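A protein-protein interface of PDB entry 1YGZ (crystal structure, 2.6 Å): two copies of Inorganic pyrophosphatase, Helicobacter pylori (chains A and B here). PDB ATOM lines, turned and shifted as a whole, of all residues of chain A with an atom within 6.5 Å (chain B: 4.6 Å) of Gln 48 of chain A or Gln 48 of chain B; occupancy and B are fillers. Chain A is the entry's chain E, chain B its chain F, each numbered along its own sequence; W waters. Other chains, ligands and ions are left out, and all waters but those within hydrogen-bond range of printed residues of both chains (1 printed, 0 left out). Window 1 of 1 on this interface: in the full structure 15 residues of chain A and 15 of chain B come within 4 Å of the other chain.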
ATOM      1  N   HIS A  24     -18.850  25.885 -19.394  1.00  0.00           N
ATOM      2  CA  HIS A  24     -18.626  25.662 -20.837  1.00  0.00           C
ATOM      3  C   HIS A  24     -17.172  25.644 -21.247  1.00  0.00           C
ATOM      4  O   HIS A  24     -16.841  25.267 -22.363  1.00  0.00           O
ATOM      5  CB  HIS A  24     -19.377  26.687 -21.673  1.00  0.00           C
ATOM      6  CG  HIS A  24     -20.863  26.577 -21.542  1.00  0.00           C
ATOM      7  ND1 HIS A  24     -21.708  27.651 -21.716  1.00  0.00           N
ATOM      8  CD2 HIS A  24     -21.651  25.516 -21.242  1.00  0.00           C
ATOM      9  CE1 HIS A  24     -22.956  27.257 -21.527  1.00  0.00           C
ATOM     10  NE2 HIS A  24     -22.949  25.967 -21.239  1.00  0.00           N
ATOM     11  N   SER A  25     -16.306  26.047 -20.333  1.00  0.00           N
ATOM     12  CA  SER A  25     -14.874  26.050 -20.583  1.00  0.00           C
ATOM     13  C   SER A  25     -14.340  24.630 -20.538  1.00  0.00           C
ATOM     14  O   SER A  25     -14.666  23.872 -19.631  1.00  0.00           O
ATOM     15  CB  SER A  25     -14.146  26.866 -19.517  1.00  0.00           C
ATOM     16  OG  SER A  25     -12.766  26.529 -19.488  1.00  0.00           O
ATOM     17  N   ASN A  26     -13.514  24.279 -21.518  1.00  0.00           N
ATOM     18  CA  ASN A  26     -12.914  22.951 -21.566  1.00  0.00           C
ATOM     19  C   ASN A  26     -11.501  23.080 -20.970  1.00  0.00           C
ATOM     20  O   ASN A  26     -10.731  22.126 -20.906  1.00  0.00           O
ATOM     21  CB  ASN A  26     -12.824  22.472 -23.002  1.00  0.00           C
ATOM     22  CG  ASN A  26     -11.714  23.136 -23.735  1.00  0.00           C
ATOM     23  OD1 ASN A  26     -11.604  24.365 -23.743  1.00  0.00           O
ATOM     24  ND2 ASN A  26     -10.860  22.333 -24.350  1.00  0.00           N
ATOM     25  N   LEU A  44      -9.393  19.564 -21.687  1.00  0.00           N
ATOM     26  CA  LEU A  44     -10.196  18.356 -21.885  1.00  0.00           C
ATOM     27  C   LEU A  44      -9.743  17.605 -23.114  1.00  0.00           C
ATOM     28  O   LEU A  44      -9.839  18.127 -24.223  1.00  0.00           O
ATOM     29  CB  LEU A  44     -11.679  18.688 -22.056  1.00  0.00           C
ATOM     30  CG  LEU A  44     -12.378  19.400 -20.903  1.00  0.00           C
ATOM     31  CD1 LEU A  44     -13.869  19.417 -21.194  1.00  0.00           C
ATOM     32  CD2 LEU A  44     -12.086  18.698 -19.573  1.00  0.00           C
ATOM     33  N   TYR A  45      -9.254  16.383 -22.903  1.00  0.00           N
ATOM     34  CA  TYR A  45      -8.790  15.528 -23.991  1.00  0.00           C
ATOM     35  C   TYR A  45      -9.920  15.214 -24.964  1.00  0.00           C
ATOM     36  O   TYR A  45      -9.684  14.997 -26.149  1.00  0.00           O
ATOM     37  CB  TYR A  45      -8.239  14.217 -23.440  1.00  0.00           C
ATOM     38  CG  TYR A  45      -6.877  14.310 -22.813  1.00  0.00           C
ATOM     39  CD1 TYR A  45      -6.477  15.449 -22.107  1.00  0.00           C
ATOM     40  CD2 TYR A  45      -6.009  13.223 -22.854  1.00  0.00           C
ATOM     41  CE1 TYR A  45      -5.240  15.494 -21.454  1.00  0.00           C
ATOM     42  CE2 TYR A  45      -4.775  13.256 -22.204  1.00  0.00           C
ATOM     43  CZ  TYR A  45      -4.405  14.386 -21.512  1.00  0.00           C
ATOM     44  OH  TYR A  45      -3.205  14.383 -20.871  1.00  0.00           O
ATOM     45  N   GLY A  46     -11.143  15.180 -24.452  1.00  0.00           N
ATOM     46  CA  GLY A  46     -12.277  14.902 -25.293  1.00  0.00           C
ATOM     47  C   GLY A  46     -13.003  16.158 -25.740  1.00  0.00           C
ATOM     48  O   GLY A  46     -12.650  17.275 -25.333  1.00  0.00           O
ATOM     49  N   ALA A  47     -14.026  15.963 -26.578  1.00  0.00           N
ATOM     50  CA  ALA A  47     -14.849  17.047 -27.124  1.00  0.00           C
ATOM     51  C   ALA A  47     -15.962  17.379 -26.158  1.00  0.00           C
ATOM     52  O   ALA A  47     -17.150  17.218 -26.479  1.00  0.00           O
ATOM     53  CB  ALA A  47     -15.447  16.630 -28.461  1.00  0.00           C
ATOM     54  N   GLN A  48     -15.565  17.838 -24.974  1.00  0.00           N
ATOM     55  CA  GLN A  48     -16.505  18.185 -23.921  1.00  0.00           C
ATOM     56  C   GLN A  48     -16.249  19.557 -23.316  1.00  0.00           C
ATOM     57  O   GLN A  48     -15.347  20.279 -23.735  1.00  0.00           O
ATOM     58  CB  GLN A  48     -16.443  17.136 -22.828  1.00  0.00           C
ATOM     59  CG  GLN A  48     -16.894  15.777 -23.274  1.00  0.00           C
ATOM     60  CD  GLN A  48     -16.608  14.730 -22.224  1.00  0.00           C
ATOM     61  OE1 GLN A  48     -15.457  14.575 -21.778  1.00  0.00           O
ATOM     62  NE2 GLN A  48     -17.645  13.992 -21.822  1.00  0.00           N
ATOM     63  N   ASN A  49     -17.051  19.900 -22.314  1.00  0.00           N
ATOM     64  CA  ASN A  49     -16.956  21.191 -21.634  1.00  0.00           C
ATOM     65  C   ASN A  49     -17.810  21.190 -20.361  1.00  0.00           C
ATOM     66  O   ASN A  49     -18.937  20.699 -20.371  1.00  0.00           O
ATOM     67  CB  ASN A  49     -17.430  22.290 -22.582  1.00  0.00           C
ATOM     68  CG  ASN A  49     -18.757  21.959 -23.224  1.00  0.00           C
ATOM     69  OD1 ASN A  49     -18.857  21.051 -24.057  1.00  0.00           O
ATOM     70  ND2 ASN A  49     -19.793  22.684 -22.827  1.00  0.00           N
ATOM     71  N   TYR A  50     -17.268  21.746 -19.277  1.00  0.00           N
ATOM     72  CA  TYR A  50     -17.960  21.790 -17.986  1.00  0.00           C
ATOM     73  C   TYR A  50     -19.420  22.207 -18.077  1.00  0.00           C
ATOM     74  O   TYR A  50     -19.770  23.133 -18.809  1.00  0.00           O
ATOM     75  CB  TYR A  50     -17.201  22.695 -17.014  1.00  0.00           C
ATOM     76  CG  TYR A  50     -15.947  22.035 -16.516  1.00  0.00           C
ATOM     77  CD1 TYR A  50     -14.803  21.982 -17.304  1.00  0.00           C
ATOM     78  CD2 TYR A  50     -15.928  21.384 -15.286  1.00  0.00           C
ATOM     79  CE1 TYR A  50     -13.663  21.288 -16.875  1.00  0.00           C
ATOM     80  CE2 TYR A  50     -14.806  20.693 -14.849  1.00  0.00           C
ATOM     81  CZ  TYR A  50     -13.679  20.644 -15.640  1.00  0.00           C
ATOM     82  OH  TYR A  50     -12.590  19.948 -15.167  1.00  0.00           O
ATOM     83  N   LYS A 132     -26.741  15.069 -17.289  1.00  0.00           N
ATOM     84  CA  LYS A 132     -25.615  15.678 -17.985  1.00  0.00           C
ATOM     85  C   LYS A 132     -24.423  15.850 -17.047  1.00  0.00           C
ATOM     86  O   LYS A 132     -23.278  15.581 -17.422  1.00  0.00           O
ATOM     87  CB  LYS A 132     -26.010  17.039 -18.566  1.00  0.00           C
ATOM     88  CG  LYS A 132     -25.021  17.592 -19.607  1.00  0.00           C
ATOM     89  CD  LYS A 132     -25.306  19.059 -19.970  1.00  0.00           C
ATOM     90  CE  LYS A 132     -26.716  19.291 -20.569  1.00  0.00           C
ATOM     91  NZ  LYS A 132     -26.908  18.844 -21.997  1.00  0.00           N
ATOM     92  N   HIS A 135     -23.107  12.120 -16.069  1.00  0.00           N
ATOM     93  CA  HIS A 135     -22.477  11.549 -17.253  1.00  0.00           C
ATOM     94  C   HIS A 135     -21.156  12.222 -17.569  1.00  0.00           C
ATOM     95  O   HIS A 135     -20.187  11.549 -17.937  1.00  0.00           O
ATOM     96  CB  HIS A 135     -23.416  11.651 -18.458  1.00  0.00           C
ATOM     97  CG  HIS A 135     -22.741  11.391 -19.764  1.00  0.00           C
ATOM     98  ND1 HIS A 135     -21.896  12.305 -20.355  1.00  0.00           N
ATOM     99  CD2 HIS A 135     -22.762  10.312 -20.582  1.00  0.00           C
ATOM    100  CE1 HIS A 135     -21.426  11.798 -21.481  1.00  0.00           C
ATOM    101  NE2 HIS A 135     -21.936  10.590 -21.642  1.00  0.00           N
ATOM    102  N   PHE A 136     -21.137  13.543 -17.436  1.00  0.00           N
ATOM    103  CA  PHE A 136     -19.938  14.330 -17.691  1.00  0.00           C
ATOM    104  C   PHE A 136     -18.809  13.803 -16.807  1.00  0.00           C
ATOM    105  O   PHE A 136     -17.800  13.282 -17.304  1.00  0.00           O
ATOM    106  CB  PHE A 136     -20.182  15.810 -17.364  1.00  0.00           C
ATOM    107  CG  PHE A 136     -18.942  16.664 -17.435  1.00  0.00           C
ATOM    108  CD1 PHE A 136     -18.480  17.145 -18.654  1.00  0.00           C
ATOM    109  CD2 PHE A 136     -18.226  16.980 -16.279  1.00  0.00           C
ATOM    110  CE1 PHE A 136     -17.321  17.933 -18.721  1.00  0.00           C
ATOM    111  CE2 PHE A 136     -17.068  17.766 -16.335  1.00  0.00           C
ATOM    112  CZ  PHE A 136     -16.616  18.243 -17.557  1.00  0.00           C
ATOM    113  N   PHE A 137     -18.995  13.920 -15.496  1.00  0.00           N
ATOM    114  CA  PHE A 137     -17.973  13.476 -14.570  1.00  0.00           C
ATOM    115  C   PHE A 137     -17.542  12.042 -14.747  1.00  0.00           C
ATOM    116  O   PHE A 137     -16.399  11.698 -14.449  1.00  0.00           O
ATOM    117  CB  PHE A 137     -18.408  13.711 -13.132  1.00  0.00           C
ATOM    118  CG  PHE A 137     -18.225  15.120 -12.697  1.00  0.00           C
ATOM    119  CD1 PHE A 137     -19.196  16.068 -12.960  1.00  0.00           C
ATOM    120  CD2 PHE A 137     -17.022  15.527 -12.126  1.00  0.00           C
ATOM    121  CE1 PHE A 137     -18.987  17.391 -12.665  1.00  0.00           C
ATOM    122  CE2 PHE A 137     -16.798  16.859 -11.825  1.00  0.00           C
ATOM    123  CZ  PHE A 137     -17.784  17.796 -12.102  1.00  0.00           C
ATOM    124  N   THR A 139     -17.138  10.528 -17.569  1.00  0.00           N
ATOM    125  CA  THR A 139     -16.644  10.329 -18.926  1.00  0.00           C
ATOM    126  C   THR A 139     -15.615  11.380 -19.330  1.00  0.00           C
ATOM    127  O   THR A 139     -14.915  11.204 -20.328  1.00  0.00           O
ATOM    128  CB  THR A 139     -17.793  10.352 -19.971  1.00  0.00           C
ATOM    129  OG1 THR A 139     -18.504  11.594 -19.896  1.00  0.00           O
ATOM    130  CG2 THR A 139     -18.769   9.239 -19.719  1.00  0.00           C
ATOM    131  N   TYR A 140     -15.505  12.461 -18.558  1.00  0.00           N
ATOM    132  CA  TYR A 140     -14.557  13.515 -18.909  1.00  0.00           C
ATOM    133  C   TYR A 140     -13.095  13.148 -18.766  1.00  0.00           C
ATOM    134  O   TYR A 140     -12.232  14.013 -18.956  1.00  0.00           O
ATOM    135  CB  TYR A 140     -14.808  14.788 -18.108  1.00  0.00           C
ATOM    136  CG  TYR A 140     -14.239  14.803 -16.711  1.00  0.00           C
ATOM    137  CD1 TYR A 140     -13.407  15.846 -16.290  1.00  0.00           C
ATOM    138  CD2 TYR A 140     -14.597  13.835 -15.778  1.00  0.00           C
ATOM    139  CE1 TYR A 140     -12.958  15.928 -14.973  1.00  0.00           C
ATOM    140  CE2 TYR A 140     -14.153  13.909 -14.460  1.00  0.00           C
ATOM    141  CZ  TYR A 140     -13.337  14.957 -14.066  1.00  0.00           C
ATOM    142  OH  TYR A 140     -12.915  15.029 -12.762  1.00  0.00           O
ATOM    143  N   LYS A 141     -12.813  11.884 -18.433  1.00  0.00           N
ATOM    144  CA  LYS A 141     -11.435  11.436 -18.289  1.00  0.00           C
ATOM    145  C   LYS A 141     -11.195  10.055 -18.893  1.00  0.00           C
ATOM    146  O   LYS A 141     -10.239   9.353 -18.530  1.00  0.00           O
ATOM    147  CB  LYS A 141     -11.004  11.459 -16.813  1.00  0.00           C
ATOM    148  CG  LYS A 141     -10.845  12.864 -16.253  1.00  0.00           C
ATOM    149  CD  LYS A 141      -9.966  12.890 -15.017  1.00  0.00           C
ATOM    150  CE  LYS A 141     -10.538  12.040 -13.886  1.00  0.00           C
ATOM    151  NZ  LYS A 141      -9.724  12.126 -12.635  1.00  0.00           N
ATOM    152  N   ASP A 142     -12.057   9.670 -19.829  1.00  0.00           N
ATOM    153  CA  ASP A 142     -11.904   8.387 -20.495  1.00  0.00           C
ATOM    154  C   ASP A 142     -10.570   8.326 -21.226  1.00  0.00           C
ATOM    155  O   ASP A 142      -9.824   7.362 -21.084  1.00  0.00           O
ATOM    156  CB  ASP A 142     -13.024   8.154 -21.505  1.00  0.00           C
ATOM    157  CG  ASP A 142     -14.371   7.955 -20.847  1.00  0.00           C
ATOM    158  OD1 ASP A 142     -14.413   7.340 -19.762  1.00  0.00           O
ATOM    159  OD2 ASP A 142     -15.391   8.394 -21.421  1.00  0.00           O
ATOM    160  N   ASN B  26     -23.216  22.584 -30.080  1.00  0.00           N
ATOM    161  CA  ASN B  26     -23.841  21.443 -29.451  1.00  0.00           C
ATOM    162  C   ASN B  26     -25.244  21.315 -30.019  1.00  0.00           C
ATOM    163  O   ASN B  26     -25.991  20.454 -29.592  1.00  0.00           O
ATOM    164  CB  ASN B  26     -23.947  21.647 -27.961  1.00  0.00           C
ATOM    165  CG  ASN B  26     -25.117  22.526 -27.597  1.00  0.00           C
ATOM    166  OD1 ASN B  26     -25.266  23.618 -28.152  1.00  0.00           O
ATOM    167  ND2 ASN B  26     -25.963  22.057 -26.668  1.00  0.00           N
ATOM    168  N   LEU B  44     -27.542  18.521 -27.845  1.00  0.00           N
ATOM    169  CA  LEU B  44     -26.787  17.502 -27.113  1.00  0.00           C
ATOM    170  C   LEU B  44     -27.241  17.368 -25.667  1.00  0.00           C
ATOM    171  O   LEU B  44     -27.111  18.295 -24.868  1.00  0.00           O
ATOM    172  CB  LEU B  44     -25.293  17.814 -27.129  1.00  0.00           C
ATOM    173  CG  LEU B  44     -24.591  17.978 -28.470  1.00  0.00           C
ATOM    174  CD1 LEU B  44     -23.067  18.059 -28.225  1.00  0.00           C
ATOM    175  CD2 LEU B  44     -24.949  16.831 -29.398  1.00  0.00           C
ATOM    176  N   GLY B  46     -25.889  15.828 -23.468  1.00  0.00           N
ATOM    177  CA  GLY B  46     -24.731  15.902 -22.595  1.00  0.00           C
ATOM    178  C   GLY B  46     -23.949  17.191 -22.721  1.00  0.00           C
ATOM    179  O   GLY B  46     -24.248  18.022 -23.582  1.00  0.00           O
ATOM    180  N   ALA B  47     -22.954  17.357 -21.853  1.00  0.00           N
ATOM    181  CA  ALA B  47     -22.105  18.547 -21.841  1.00  0.00           C
ATOM    182  C   ALA B  47     -20.997  18.408 -22.874  1.00  0.00           C
ATOM    183  O   ALA B  47     -19.809  18.458 -22.543  1.00  0.00           O
ATOM    184  CB  ALA B  47     -21.495  18.741 -20.454  1.00  0.00           C
ATOM    185  N   GLN B  48     -21.397  18.229 -24.130  1.00  0.00           N
ATOM    186  CA  GLN B  48     -20.445  18.067 -25.223  1.00  0.00           C
ATOM    187  C   GLN B  48     -20.657  19.041 -26.380  1.00  0.00           C
ATOM    188  O   GLN B  48     -21.515  19.920 -26.328  1.00  0.00           O
ATOM    189  CB  GLN B  48     -20.517  16.645 -25.759  1.00  0.00           C
ATOM    190  CG  GLN B  48     -20.120  15.584 -24.762  1.00  0.00           C
ATOM    191  CD  GLN B  48     -20.427  14.184 -25.265  1.00  0.00           C
ATOM    192  OE1 GLN B  48     -21.580  13.861 -25.581  1.00  0.00           O
ATOM    193  NE2 GLN B  48     -19.396  13.342 -25.343  1.00  0.00           N
ATOM    194  N   ASN B  49     -19.863  18.868 -27.427  1.00  0.00           N
ATOM    195  CA  ASN B  49     -19.943  19.718 -28.599  1.00  0.00           C
ATOM    196  C   ASN B  49     -19.119  19.122 -29.730  1.00  0.00           C
ATOM    197  O   ASN B  49     -18.011  18.636 -29.497  1.00  0.00           O
ATOM    198  CB  ASN B  49     -19.425  21.106 -28.266  1.00  0.00           C
ATOM    199  CG  ASN B  49     -18.079  21.074 -27.580  1.00  0.00           C
ATOM    200  OD1 ASN B  49     -17.964  20.677 -26.413  1.00  0.00           O
ATOM    201  ND2 ASN B  49     -17.044  21.492 -28.302  1.00  0.00           N
ATOM    202  N   HIS B 135     -14.164   8.920 -29.572  1.00  0.00           N
ATOM    203  CA  HIS B 135     -14.813   8.969 -28.266  1.00  0.00           C
ATOM    204  C   HIS B 135     -16.108   9.776 -28.295  1.00  0.00           C
ATOM    205  O   HIS B 135     -17.141   9.377 -27.731  1.00  0.00           O
ATOM    206  CB  HIS B 135     -13.847   9.559 -27.235  1.00  0.00           C
ATOM    207  CG  HIS B 135     -14.503   9.937 -25.945  1.00  0.00           C
ATOM    208  ND1 HIS B 135     -15.302  11.054 -25.818  1.00  0.00           N
ATOM    209  CD2 HIS B 135     -14.477   9.351 -24.727  1.00  0.00           C
ATOM    210  CE1 HIS B 135     -15.733  11.143 -24.572  1.00  0.00           C
ATOM    211  NE2 HIS B 135     -15.245  10.123 -23.890  1.00  0.00           N
ATOM    212  N   PHE B 136     -16.043  10.926 -28.946  1.00  0.00           N
ATOM    213  CA  PHE B 136     -17.207  11.785 -29.064  1.00  0.00           C
ATOM    214  C   PHE B 136     -18.365  10.934 -29.551  1.00  0.00           C
ATOM    215  O   PHE B 136     -19.298  10.670 -28.790  1.00  0.00           O
ATOM    216  CB  PHE B 136     -16.942  12.903 -30.068  1.00  0.00           C
ATOM    217  CG  PHE B 136     -18.150  13.743 -30.379  1.00  0.00           C
ATOM    218  CD1 PHE B 136     -18.583  14.727 -29.482  1.00  0.00           C
ATOM    219  CD2 PHE B 136     -18.865  13.543 -31.569  1.00  0.00           C
ATOM    220  CE1 PHE B 136     -19.708  15.511 -29.758  1.00  0.00           C
ATOM    221  CE2 PHE B 136     -20.000  14.322 -31.864  1.00  0.00           C
ATOM    222  CZ  PHE B 136     -20.424  15.308 -30.957  1.00  0.00           C
ATOM    223  N   THR B 139     -20.127   8.386 -27.459  1.00  0.00           N
ATOM    224  CA  THR B 139     -20.634   8.821 -26.162  1.00  0.00           C
ATOM    225  C   THR B 139     -21.595   9.989 -26.301  1.00  0.00           C
ATOM    226  O   THR B 139     -22.255  10.353 -25.339  1.00  0.00           O
ATOM    227  CB  THR B 139     -19.509   9.267 -25.196  1.00  0.00           C
ATOM    228  OG1 THR B 139     -18.784  10.363 -25.766  1.00  0.00           O
ATOM    229  CG2 THR B 139     -18.552   8.118 -24.915  1.00  0.00           C
ATOM    230  N   TYR B 140     -21.693  10.572 -27.491  1.00  0.00           N
ATOM    231  CA  TYR B 140     -22.575  11.711 -27.645  1.00  0.00           C
ATOM    232  C   TYR B 140     -24.063  11.384 -27.575  1.00  0.00           C
ATOM    233  O   TYR B 140     -24.887  12.272 -27.714  1.00  0.00           O
ATOM    234  CB  TYR B 140     -22.255  12.466 -28.944  1.00  0.00           C
ATOM    235  CG  TYR B 140     -22.848  11.895 -30.210  1.00  0.00           C
ATOM    236  CD1 TYR B 140     -23.658  12.683 -31.031  1.00  0.00           C
ATOM    237  CD2 TYR B 140     -22.554  10.600 -30.624  1.00  0.00           C
ATOM    238  CE1 TYR B 140     -24.152  12.206 -32.235  1.00  0.00           C
ATOM    239  CE2 TYR B 140     -23.049  10.111 -31.830  1.00  0.00           C
ATOM    240  CZ  TYR B 140     -23.847  10.923 -32.633  1.00  0.00           C
ATOM    241  OH  TYR B 140     -24.330  10.473 -33.840  1.00  0.00           O
HETATM  242  O   HOH W   1     -24.153  11.497 -22.935  1.00  0.00           O
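Among the printed residues, merely in contact across the chains: Lys 132 of chain A with Ala 47 of chain B (3.1 Å), Ala 47 of chain A with Gln 48 of chain B (3.5 Å), Gln 48 of chain A with Gln 48 of chain B (3.6 Å), Asn 49 of chain A with Gln 48 of chain B (3.6 Å), Gln 48 of chain A with Ala 47 of chain B (3.6 Å), Gln 48 of chain A with Asn 49 of chain B (3.7 Å), His 135 of chain A with Thr 139 of chain B (3.7 Å), Thr 139 of chain A with His 135 of chain B (3.7 Å), Ala 47 of chain A with Phe 136 of chain B (3.8 Å) and Phe 136 of chain A with Ala 47 of chain B (3.9 Å).
The backbone carbonyl oxygen (O) of Ala 47 of chain A is in hydrogen-bond range of the backbone NH (N) of Asn 49 of chain B. O of Ala 47 of chain B lies within hydrogen-bond range of N of Asn 49 of chain A, 3.1 Å away. OD1 of Asn 49 of chain A lies close to OD1 of Asn 49 of chain B (2.5 Å). The side-chain amino group (NZ) of Lys 132 of chain A sits at hydrogen-bond distance from the backbone carbonyl oxygen (O) of Leu 44 of chain B. O of Gly 46 of chain B lies within hydrogen-bond range of NZ of Lys 132 of chain A (3.2 Å). The side-chain carboxylate of Asp 142 of chain A sits at hydrogen-bond distance from a ring nitrogen (NE2) of His 135 of chain B (3.0 Å).
Ala 47 of chain A touches Asn 49 of chain B, and with the chains exchanged Asn 49 of chain A touches Ala 47 of chain B. Gln 48 of chain A touches Asn 49 of chain B, and with the chains exchanged Asn 49 of chain A touches Gln 48 of chain B. Asn 49 of chain A touches its own counterpart, Asn 49 of chain B. His 135 of chain A touches Thr 139 of chain B, and with the chains exchanged Thr 139 of chain A touches His 135 of chain B. Of the 16 pairs that touch across the chains among the printed residues, 12 have their exchanged pair printed and touching as well.
Printed residues of chain B within 4 Å of Gln 48 of chain A: Ala 47, Gln 48 and Asn 49. Gln 48 of chain B touches three residues of chain A. Printed residues of chain B within 4 Å of Asp 142 of chain A: His 135 (3.0 Å). Of the printed residues of chain B, Ala 47 of chain A touches Gln 48 (3.5 Å), Asn 49 (3.3 Å) and Phe 136 (3.8 Å). Tyr 140 of chain A touches none of the printed residues of chain B. His 24 of chain A touches none of the printed residues of chain B. The nearest residue of chain A that does not touch Gln 48 of chain B is His 135 of chain A (4.6 Å).
Hydrophobic or aromatic side chains of chain A that line the printed part of chain B: Ala 47, His 135 and Phe 136. Along chain A the printed residues that touch a printed residue of chain B span positions 47 to 142. Hydrophobic or aromatic side chains of chain B within 4 Å of the printed part of chain A: Ala 47, His 135 and Phe 136. Among the printed residues, 16 pairs touch across the chains.
The side-chain hydroxyl (OG1) of Thr 139 of chain A lies within hydrogen-bond range of the side-chain amide nitrogen (NE2) of Gln 48 of chain A (3.2 Å). O of His 135 of chain A sits at hydrogen-bond distance from OG1 of Thr 139 of chain A. O of Asn 26 of chain B sits at hydrogen-bond distance from N of Leu 44 of chain B, at 3.0 Å. The side-chain hydroxyl (OG1) of Thr 139 of chain B is in hydrogen-bond range of the side-chain amide nitrogen (NE2) of Gln 48 of chain B, 3.1 Å away. OG1 of Thr 139 of chain B is in hydrogen-bond range of O of His 135 of chain B (2.7 Å). The backbone carbonyl oxygen (O) of Phe 136 of chain B sits at hydrogen-bond distance from the side-chain hydroxyl (OG1) of Thr 139 of chain B (3.1 Å).
Water W1 lies within hydrogen-bond range of NE2 of His 135 of chain A (2.7 Å) and O of Thr 139 of chain B (3.3 Å).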
